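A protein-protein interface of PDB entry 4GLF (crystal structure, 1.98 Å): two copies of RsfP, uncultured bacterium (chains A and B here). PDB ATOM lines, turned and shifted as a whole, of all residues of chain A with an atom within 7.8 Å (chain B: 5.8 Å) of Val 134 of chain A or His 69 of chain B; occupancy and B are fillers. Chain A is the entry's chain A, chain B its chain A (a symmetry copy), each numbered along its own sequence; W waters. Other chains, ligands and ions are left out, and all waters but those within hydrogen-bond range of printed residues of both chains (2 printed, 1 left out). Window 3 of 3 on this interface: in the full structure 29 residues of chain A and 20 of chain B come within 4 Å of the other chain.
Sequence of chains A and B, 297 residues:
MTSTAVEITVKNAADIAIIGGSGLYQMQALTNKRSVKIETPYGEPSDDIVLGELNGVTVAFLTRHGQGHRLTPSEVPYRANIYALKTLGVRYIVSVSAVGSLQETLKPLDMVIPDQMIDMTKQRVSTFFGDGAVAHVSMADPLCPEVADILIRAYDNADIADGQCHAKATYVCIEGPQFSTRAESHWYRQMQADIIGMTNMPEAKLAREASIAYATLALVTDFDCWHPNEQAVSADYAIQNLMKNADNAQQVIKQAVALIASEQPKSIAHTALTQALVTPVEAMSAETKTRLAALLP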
ATOM      1  N   THR A 127      14.606 -27.549  16.763  1.00  0.00           N
ATOM      2  CA  THR A 127      14.274 -27.022  15.423  1.00  0.00           C
ATOM      3  C   THR A 127      15.492 -27.122  14.547  1.00  0.00           C
ATOM      4  O   THR A 127      16.640 -27.175  15.038  1.00  0.00           O
ATOM      5  CB  THR A 127      13.826 -25.501  15.496  1.00  0.00           C
ATOM      6  OG1 THR A 127      13.530 -24.984  14.193  1.00  0.00           O
ATOM      7  CG2 THR A 127      14.879 -24.560  16.143  1.00  0.00           C
ATOM      8  N   PHE A 128      15.244 -27.120  13.225  1.00  0.00           N
ATOM      9  CA  PHE A 128      16.329 -27.007  12.294  1.00  0.00           C
ATOM     10  C   PHE A 128      16.624 -25.549  12.022  1.00  0.00           C
ATOM     11  O   PHE A 128      17.609 -25.255  11.346  1.00  0.00           O
ATOM     12  CB  PHE A 128      15.978 -27.659  10.949  1.00  0.00           C
ATOM     13  CG  PHE A 128      15.947 -29.156  10.991  1.00  0.00           C
ATOM     14  CD1 PHE A 128      17.139 -29.905  11.027  1.00  0.00           C
ATOM     15  CD2 PHE A 128      14.759 -29.835  10.813  1.00  0.00           C
ATOM     16  CE1 PHE A 128      17.119 -31.300  10.998  1.00  0.00           C
ATOM     17  CE2 PHE A 128      14.729 -31.220  10.746  1.00  0.00           C
ATOM     18  CZ  PHE A 128      15.912 -31.969  10.860  1.00  0.00           C
ATOM     19  N   PHE A 129      15.703 -24.653  12.426  1.00  0.00           N
ATOM     20  CA  PHE A 129      15.810 -23.233  12.076  1.00  0.00           C
ATOM     21  C   PHE A 129      16.634 -22.376  13.070  1.00  0.00           C
ATOM     22  O   PHE A 129      17.102 -22.884  14.079  1.00  0.00           O
ATOM     23  CB  PHE A 129      14.381 -22.688  11.786  1.00  0.00           C
ATOM     24  CG  PHE A 129      13.812 -23.337  10.535  1.00  0.00           C
ATOM     25  CD1 PHE A 129      13.156 -24.563  10.598  1.00  0.00           C
ATOM     26  CD2 PHE A 129      14.074 -22.790   9.275  1.00  0.00           C
ATOM     27  CE1 PHE A 129      12.698 -25.227   9.452  1.00  0.00           C
ATOM     28  CE2 PHE A 129      13.630 -23.434   8.124  1.00  0.00           C
ATOM     29  CZ  PHE A 129      12.976 -24.706   8.209  1.00  0.00           C
ATOM     30  N   GLY A 130      16.822 -21.092  12.787  1.00  0.00           N
ATOM     31  CA  GLY A 130      17.770 -20.268  13.540  1.00  0.00           C
ATOM     32  C   GLY A 130      19.000 -20.131  12.646  1.00  0.00           C
ATOM     33  O   GLY A 130      19.070 -20.730  11.554  1.00  0.00           O
ATOM     34  N   ASP A 131      19.946 -19.318  13.113  1.00  0.00           N
ATOM     35  CA  ASP A 131      21.207 -19.035  12.442  1.00  0.00           C
ATOM     36  C   ASP A 131      21.058 -18.821  10.948  1.00  0.00           C
ATOM     37  O   ASP A 131      21.763 -19.499  10.140  1.00  0.00           O
ATOM     38  CB  ASP A 131      22.246 -20.129  12.754  1.00  0.00           C
ATOM     39  CG  ASP A 131      23.667 -19.695  12.423  1.00  0.00           C
ATOM     40  OD1 ASP A 131      24.036 -18.489  12.520  1.00  0.00           O
ATOM     41  OD2 ASP A 131      24.439 -20.578  12.044  1.00  0.00           O
ATOM     42  N   GLY A 132      20.177 -17.882  10.554  1.00  0.00           N
ATOM     43  CA  GLY A 132      20.051 -17.520   9.111  1.00  0.00           C
ATOM     44  C   GLY A 132      18.723 -17.890   8.412  1.00  0.00           C
ATOM     45  O   GLY A 132      18.479 -17.514   7.256  1.00  0.00           O
ATOM     46  N   ALA A 133      17.859 -18.611   9.090  1.00  0.00           N
ATOM     47  CA  ALA A 133      16.522 -18.943   8.535  1.00  0.00           C
ATOM     48  C   ALA A 133      15.484 -19.053   9.678  1.00  0.00           C
ATOM     49  O   ALA A 133      15.764 -19.592  10.783  1.00  0.00           O
ATOM     50  CB  ALA A 133      16.556 -20.244   7.727  1.00  0.00           C
ATOM     51  N   VAL A 134      14.297 -18.520   9.421  1.00  0.00           N
ATOM     52  CA  VAL A 134      13.182 -18.502  10.374  1.00  0.00           C
ATOM     53  C   VAL A 134      11.970 -19.218   9.762  1.00  0.00           C
ATOM     54  O   VAL A 134      11.642 -18.983   8.577  1.00  0.00           O
ATOM     55  CB  VAL A 134      12.851 -17.016  10.657  1.00  0.00           C
ATOM     56  CG1 VAL A 134      11.512 -16.893  11.387  1.00  0.00           C
ATOM     57  CG2 VAL A 134      13.982 -16.351  11.486  1.00  0.00           C
ATOM     58  N   ALA A 135      11.379 -20.182  10.485  1.00  0.00           N
ATOM     59  CA  ALA A 135      10.121 -20.860  10.046  1.00  0.00           C
ATOM     60  C   ALA A 135       9.354 -21.199  11.313  1.00  0.00           C
ATOM     61  O   ALA A 135       9.963 -21.458  12.381  1.00  0.00           O
ATOM     62  CB  ALA A 135      10.439 -22.149   9.243  1.00  0.00           C
ATOM     63  N   HIS A 136       8.024 -21.221  11.217  1.00  0.00           N
ATOM     64  CA  HIS A 136       7.128 -21.529  12.358  1.00  0.00           C
ATOM     65  C   HIS A 136       6.102 -22.523  11.899  1.00  0.00           C
ATOM     66  O   HIS A 136       5.047 -22.111  11.463  1.00  0.00           O
ATOM     67  CB  HIS A 136       6.432 -20.229  12.839  1.00  0.00           C
ATOM     68  CG  HIS A 136       7.379 -19.213  13.430  1.00  0.00           C
ATOM     69  ND1 HIS A 136       7.921 -19.359  14.678  1.00  0.00           N
ATOM     70  CD2 HIS A 136       7.886 -18.055  12.912  1.00  0.00           C
ATOM     71  CE1 HIS A 136       8.738 -18.311  14.905  1.00  0.00           C
ATOM     72  NE2 HIS A 136       8.715 -17.523  13.818  1.00  0.00           N
ATOM     73  N   VAL A 137       6.387 -23.837  11.963  1.00  0.00           N
ATOM     74  CA  VAL A 137       5.397 -24.820  11.554  1.00  0.00           C
ATOM     75  C   VAL A 137       4.335 -24.970  12.653  1.00  0.00           C
ATOM     76  O   VAL A 137       4.563 -24.631  13.814  1.00  0.00           O
ATOM     77  CB  VAL A 137       6.010 -26.173  11.149  1.00  0.00           C
ATOM     78  CG1 VAL A 137       7.019 -25.918  10.019  1.00  0.00           C
ATOM     79  CG2 VAL A 137       6.723 -26.868  12.360  1.00  0.00           C
ATOM     80  N   LEU A 273       6.148 -27.173   5.552  1.00  0.00           N
ATOM     81  CA  LEU A 273       7.078 -26.091   5.373  1.00  0.00           C
ATOM     82  C   LEU A 273       6.628 -24.932   4.510  1.00  0.00           C
ATOM     83  O   LEU A 273       6.985 -23.794   4.802  1.00  0.00           O
ATOM     84  CB  LEU A 273       8.492 -26.578   5.010  1.00  0.00           C
ATOM     85  CG  LEU A 273       9.583 -25.624   5.529  1.00  0.00           C
ATOM     86  CD1 LEU A 273       9.426 -25.369   7.035  1.00  0.00           C
ATOM     87  CD2 LEU A 273      10.968 -26.176   5.245  1.00  0.00           C
ATOM     88  N   ALA A 276       4.895 -22.013   6.317  1.00  0.00           N
ATOM     89  CA  ALA A 276       5.573 -21.726   7.580  1.00  0.00           C
ATOM     90  C   ALA A 276       6.885 -20.916   7.460  1.00  0.00           C
ATOM     91  O   ALA A 276       7.341 -20.281   8.423  1.00  0.00           O
ATOM     92  CB  ALA A 276       5.854 -23.060   8.267  1.00  0.00           C
ATOM     93  N   LEU A 277       7.501 -20.928   6.263  1.00  0.00           N
ATOM     94  CA  LEU A 277       8.828 -20.346   6.065  1.00  0.00           C
ATOM     95  C   LEU A 277       8.740 -18.862   5.973  1.00  0.00           C
ATOM     96  O   LEU A 277       8.062 -18.347   5.095  1.00  0.00           O
ATOM     97  CB  LEU A 277       9.472 -20.910   4.781  1.00  0.00           C
ATOM     98  CG  LEU A 277      10.955 -20.615   4.469  1.00  0.00           C
ATOM     99  CD1 LEU A 277      11.942 -21.076   5.571  1.00  0.00           C
ATOM    100  CD2 LEU A 277      11.334 -21.204   3.073  1.00  0.00           C
ATOM    101  N   VAL A 278       9.451 -18.155   6.845  1.00  0.00           N
ATOM    102  CA  VAL A 278       9.410 -16.687   6.890  1.00  0.00           C
ATOM    103  C   VAL A 278      10.547 -16.146   6.028  1.00  0.00           C
ATOM    104  O   VAL A 278      10.338 -15.195   5.279  1.00  0.00           O
ATOM    105  CB  VAL A 278       9.506 -16.135   8.330  1.00  0.00           C
ATOM    106  CG1 VAL A 278       9.545 -14.608   8.365  1.00  0.00           C
ATOM    107  CG2 VAL A 278       8.327 -16.639   9.189  1.00  0.00           C
ATOM    108  N   THR A 279      11.714 -16.785   6.047  1.00  0.00           N
ATOM    109  CA  THR A 279      12.880 -16.247   5.311  1.00  0.00           C
ATOM    110  C   THR A 279      12.797 -16.840   3.948  1.00  0.00           C
ATOM    111  O   THR A 279      12.924 -18.051   3.825  1.00  0.00           O
ATOM    112  CB  THR A 279      14.200 -16.759   5.918  1.00  0.00           C
ATOM    113  OG1 THR A 279      14.243 -16.447   7.313  1.00  0.00           O
ATOM    114  CG2 THR A 279      15.458 -16.260   5.123  1.00  0.00           C
ATOM    115  N   PRO A 280      12.579 -16.009   2.917  1.00  0.00           N
ATOM    116  CA  PRO A 280      12.604 -16.681   1.602  1.00  0.00           C
ATOM    117  C   PRO A 280      13.975 -17.288   1.280  1.00  0.00           C
ATOM    118  O   PRO A 280      15.018 -16.731   1.669  1.00  0.00           O
ATOM    119  CB  PRO A 280      12.254 -15.578   0.603  1.00  0.00           C
ATOM    120  CG  PRO A 280      12.128 -14.297   1.388  1.00  0.00           C
ATOM    121  CD  PRO A 280      12.451 -14.548   2.847  1.00  0.00           C
ATOM    122  N   MET A 284      18.524 -16.387   2.040  1.00  0.00           N
ATOM    123  CA  MET A 284      19.405 -17.181   2.910  1.00  0.00           C
ATOM    124  C   MET A 284      20.848 -17.068   2.469  1.00  0.00           C
ATOM    125  O   MET A 284      21.123 -17.006   1.287  1.00  0.00           O
ATOM    126  CB  MET A 284      19.005 -18.628   2.894  1.00  0.00           C
ATOM    127  CG  MET A 284      17.649 -18.832   3.590  1.00  0.00           C
ATOM    128  SD  MET A 284      17.160 -20.506   3.222  1.00  0.00           S
ATOM    129  CE  MET A 284      15.485 -20.616   3.937  1.00  0.00           C
ATOM    130  N   THR A 288      23.614 -21.303   5.085  1.00  0.00           N
ATOM    131  CA  THR A 288      22.263 -21.667   5.539  1.00  0.00           C
ATOM    132  C   THR A 288      21.526 -22.589   4.553  1.00  0.00           C
ATOM    133  O   THR A 288      21.033 -23.650   4.958  1.00  0.00           O
ATOM    134  CB  THR A 288      21.479 -20.367   5.829  1.00  0.00           C
ATOM    135  OG1 THR A 288      22.183 -19.675   6.902  1.00  0.00           O
ATOM    136  CG2 THR A 288      20.008 -20.712   6.238  1.00  0.00           C
ATOM    137  N   LEU A 292      20.401 -26.541   5.172  1.00  0.00           N
ATOM    138  CA  LEU A 292      18.973 -26.857   5.151  1.00  0.00           C
ATOM    139  C   LEU A 292      18.534 -27.564   3.883  1.00  0.00           C
ATOM    140  O   LEU A 292      17.339 -27.739   3.677  1.00  0.00           O
ATOM    141  CB  LEU A 292      18.104 -25.595   5.298  1.00  0.00           C
ATOM    142  CG  LEU A 292      18.318 -24.804   6.644  1.00  0.00           C
ATOM    143  CD1 LEU A 292      17.471 -23.535   6.662  1.00  0.00           C
ATOM    144  CD2 LEU A 292      18.035 -25.679   7.875  1.00  0.00           C
ATOM    145  N   HIS B  65      13.498  -8.729  16.035  1.00  0.00           N
ATOM    146  CA  HIS B  65      13.940  -9.858  15.182  1.00  0.00           C
ATOM    147  C   HIS B  65      14.965  -9.533  14.120  1.00  0.00           C
ATOM    148  O   HIS B  65      15.280 -10.407  13.304  1.00  0.00           O
ATOM    149  CB  HIS B  65      12.751 -10.538  14.528  1.00  0.00           C
ATOM    150  CG  HIS B  65      11.858 -11.210  15.534  1.00  0.00           C
ATOM    151  ND1 HIS B  65      12.121 -12.431  16.065  1.00  0.00           N
ATOM    152  CD2 HIS B  65      10.719 -10.731  16.193  1.00  0.00           C
ATOM    153  CE1 HIS B  65      11.162 -12.735  16.973  1.00  0.00           C
ATOM    154  NE2 HIS B  65      10.300 -11.694  17.033  1.00  0.00           N
ATOM    155  N   GLY B  66      15.475  -8.294  14.147  1.00  0.00           N
ATOM    156  CA  GLY B  66      16.477  -7.810  13.196  1.00  0.00           C
ATOM    157  C   GLY B  66      15.800  -7.387  11.887  1.00  0.00           C
ATOM    158  O   GLY B  66      14.604  -7.636  11.690  1.00  0.00           O
ATOM    159  N   GLN B  67      16.557  -6.765  10.987  1.00  0.00           N
ATOM    160  CA  GLN B  67      15.956  -6.344   9.690  1.00  0.00           C
ATOM    161  C   GLN B  67      15.669  -7.585   8.863  1.00  0.00           C
ATOM    162  O   GLN B  67      16.388  -8.625   8.959  1.00  0.00           O
ATOM    163  CB  GLN B  67      16.826  -5.284   8.963  1.00  0.00           C
ATOM    164  CG  GLN B  67      16.227  -4.658   7.699  1.00  0.00           C
ATOM    165  CD  GLN B  67      14.723  -4.324   7.758  1.00  0.00           C
ATOM    166  OE1 GLN B  67      13.986  -4.727   8.676  1.00  0.00           O
ATOM    167  NE2 GLN B  67      14.254  -3.610   6.733  1.00  0.00           N
ATOM    168  N   GLY B  68      14.559  -7.508   8.136  1.00  0.00           N
ATOM    169  CA  GLY B  68      14.027  -8.631   7.378  1.00  0.00           C
ATOM    170  C   GLY B  68      13.574  -9.779   8.264  1.00  0.00           C
ATOM    171  O   GLY B  68      13.420 -10.900   7.788  1.00  0.00           O
ATOM    172  N   HIS B  69      13.321  -9.514   9.549  1.00  0.00           N
ATOM    173  CA  HIS B  69      12.872 -10.541  10.449  1.00  0.00           C
ATOM    174  C   HIS B  69      13.813 -11.730  10.415  1.00  0.00           C
ATOM    175  O   HIS B  69      13.415 -12.851  10.179  1.00  0.00           O
ATOM    176  CB  HIS B  69      11.423 -10.945  10.117  1.00  0.00           C
ATOM    177  CG  HIS B  69      10.689 -11.488  11.301  1.00  0.00           C
ATOM    178  ND1 HIS B  69      11.055 -12.663  11.926  1.00  0.00           N
ATOM    179  CD2 HIS B  69       9.636 -10.949  12.055  1.00  0.00           C
ATOM    180  CE1 HIS B  69      10.243 -12.868  12.990  1.00  0.00           C
ATOM    181  NE2 HIS B  69       9.377 -11.816  13.068  1.00  0.00           N
ATOM    182  N   ARG B  70      15.090 -11.509  10.653  1.00  0.00           N
ATOM    183  CA  ARG B  70      16.038 -12.606  10.448  1.00  0.00           C
ATOM    184  C   ARG B  70      16.286 -13.525  11.640  1.00  0.00           C
ATOM    185  O   ARG B  70      17.008 -14.473  11.498  1.00  0.00           O
ATOM    186  CB  ARG B  70      17.356 -12.009   9.991  1.00  0.00           C
ATOM    187  CG  ARG B  70      17.926 -11.046  11.016  1.00  0.00           C
ATOM    188  CD  ARG B  70      19.162 -10.227  10.528  1.00  0.00           C
ATOM    189  NE  ARG B  70      19.696  -9.524  11.709  1.00  0.00           N
ATOM    190  CZ  ARG B  70      20.550 -10.075  12.581  1.00  0.00           C
ATOM    191  NH1 ARG B  70      21.052 -11.273  12.314  1.00  0.00           N
ATOM    192  NH2 ARG B  70      20.914  -9.438  13.709  1.00  0.00           N
ATOM    193  N   LEU B  71      15.737 -13.234  12.825  1.00  0.00           N
ATOM    194  CA  LEU B  71      16.044 -14.045  14.056  1.00  0.00           C
ATOM    195  C   LEU B  71      14.814 -14.786  14.536  1.00  0.00           C
ATOM    196  O   LEU B  71      13.705 -14.238  14.426  1.00  0.00           O
ATOM    197  CB  LEU B  71      16.524 -13.132  15.203  1.00  0.00           C
ATOM    198  CG  LEU B  71      17.770 -12.300  14.812  1.00  0.00           C
ATOM    199  CD1 LEU B  71      17.992 -11.229  15.905  1.00  0.00           C
ATOM    200  CD2 LEU B  71      18.990 -13.219  14.638  1.00  0.00           C
ATOM    201  N   THR B  72      14.978 -16.030  14.969  1.00  0.00           N
ATOM    202  CA  THR B  72      13.927 -16.742  15.692  1.00  0.00           C
ATOM    203  C   THR B  72      13.931 -16.233  17.153  1.00  0.00           C
ATOM    204  O   THR B  72      14.911 -15.649  17.596  1.00  0.00           O
ATOM    205  CB  THR B  72      14.193 -18.269  15.755  1.00  0.00           C
ATOM    206  OG1 THR B  72      15.365 -18.532  16.523  1.00  0.00           O
ATOM    207  CG2 THR B  72      14.330 -18.879  14.339  1.00  0.00           C
ATOM    208  N   GLU B  75      16.767 -17.126  19.566  1.00  0.00           N
ATOM    209  CA  GLU B  75      18.144 -16.641  19.375  1.00  0.00           C
ATOM    210  C   GLU B  75      18.239 -15.110  19.534  1.00  0.00           C
ATOM    211  O   GLU B  75      19.285 -14.561  19.382  1.00  0.00           O
ATOM    212  CB  GLU B  75      18.710 -17.119  18.020  1.00  0.00           C
ATOM    213  CG  GLU B  75      18.136 -16.386  16.820  1.00  0.00           C
ATOM    214  CD  GLU B  75      18.471 -17.153  15.503  1.00  0.00           C
ATOM    215  OE1 GLU B  75      19.454 -17.939  15.464  1.00  0.00           O
ATOM    216  OE2 GLU B  75      17.794 -16.942  14.521  1.00  0.00           O
HETATM  217  O   HOH W   1      13.922 -14.106   7.782  1.00  0.00           O
HETATM  218  O   HOH W   2      18.685 -16.423  12.222  1.00  0.00           O
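The backbone NH of Asp 131 of chain A lies within hydrogen-bond range of the side-chain carboxylate of Glu 75 of chain B (2.8 Å).
The side-chain hydroxyl (OG1) of Thr 279 of chain A is in hydrogen-bond range of the backbone NH (N) of Val 134 of chain A (3.0 Å). OG1 of Thr 288 of chain A is in hydrogen-bond range of O of Asp 131 of chain A (3.3 Å). The backbone NH (N) of Val 278 of chain A sits at hydrogen-bond distance from the backbone carbonyl oxygen (O) of Val 134 of chain A, 2.9 Å away. The backbone carbonyl oxygen of His 65 of chain B is in hydrogen-bond range of the backbone NH of Arg 70 of chain B, at 2.9 Å. The backbone NH (N) of Thr 72 of chain B lies within hydrogen-bond range of the side-chain carboxylate (OE2) of Glu 75 of chain B. O of His 65 of chain B sits at hydrogen-bond distance from N of Leu 71 of chain B, 2.9 Å away.
Among the printed residues, pairs that only touch across the chains: Gly 130 of chain A with Thr 72 of chain B, Gly 130 of chain A with Glu 75 of chain B, Ala 133 of chain A with Thr 72 of chain B, Val 134 of chain A with His 69 of chain B, Val 134 of chain A with Arg 70 of chain B, Val 134 of chain A with Leu 71 of chain B and Val 134 of chain A with Thr 72 of chain B.
Printed residues of chain B within 4 Å of Ala 133 of chain A: Thr 72. Of chain B, only His 69 (3.8 Å), Arg 70 (3.6 Å), Leu 71 (3.5 Å) and Thr 72 (3.6 Å) come within 4 Å of Val 134 of chain A. No residue of chain A comes within 4 Å of Gly 68 of chain B. His 69 of chain B touches just one residue of chain A: Val 134 (3.8 Å). Printed residues of chain A within 4 Å of Arg 70 of chain B: Val 134 (3.6 Å). Printed residues of chain A within 4 Å of Leu 71 of chain B: Val 134 (3.5 Å). Printed residues of chain A within 4 Å of Glu 75 of chain B: Gly 130 (3.5 Å) and Asp 131 (2.8 Å). The nearest residue of chain B that does not touch Val 134 of chain A is Glu 75 of chain B (4.9 Å). The nearest residue of chain A that does not touch His 69 of chain B is Val 278 of chain A (4.3 Å). The nearest printed residue of chain A that does not touch Thr 72 of chain B is Phe 129 of chain A (4.4 Å).
Of the 20 printed residues of chain A, 4 touch a printed residue of chain B. Hydrophobic or aromatic side chains of chain A that line the printed part of chain B: Val 134. Of the 9 printed residues of chain B, 5 touch a printed residue of chain A. Among the printed residues, 8 pairs touch across the chains. Among the printed residues, no Asp or Glu carboxylate lies within 4 Å of a Lys or Arg side-chain nitrogen of the other chain.
No position is printed for both chains. Of the 8 pairs that touch across the chains among the printed residues, none has its exchanged pair printed and touching as well.
Water W1 lies within hydrogen-bond range of OG1 of Thr 279 of chain A (2.4 Å), O of His 69 of chain B (2.8 Å) and O of Gly 68 of chain B (3.2 Å). Water W2 lies within hydrogen-bond range of the side-chain carboxylate of Glu 75 of chain B, the backbone NH of Gly 132 of chain A, the backbone carbonyl oxygen of Arg 70 of chain B and the backbone NH of Asp 131 of chain A.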
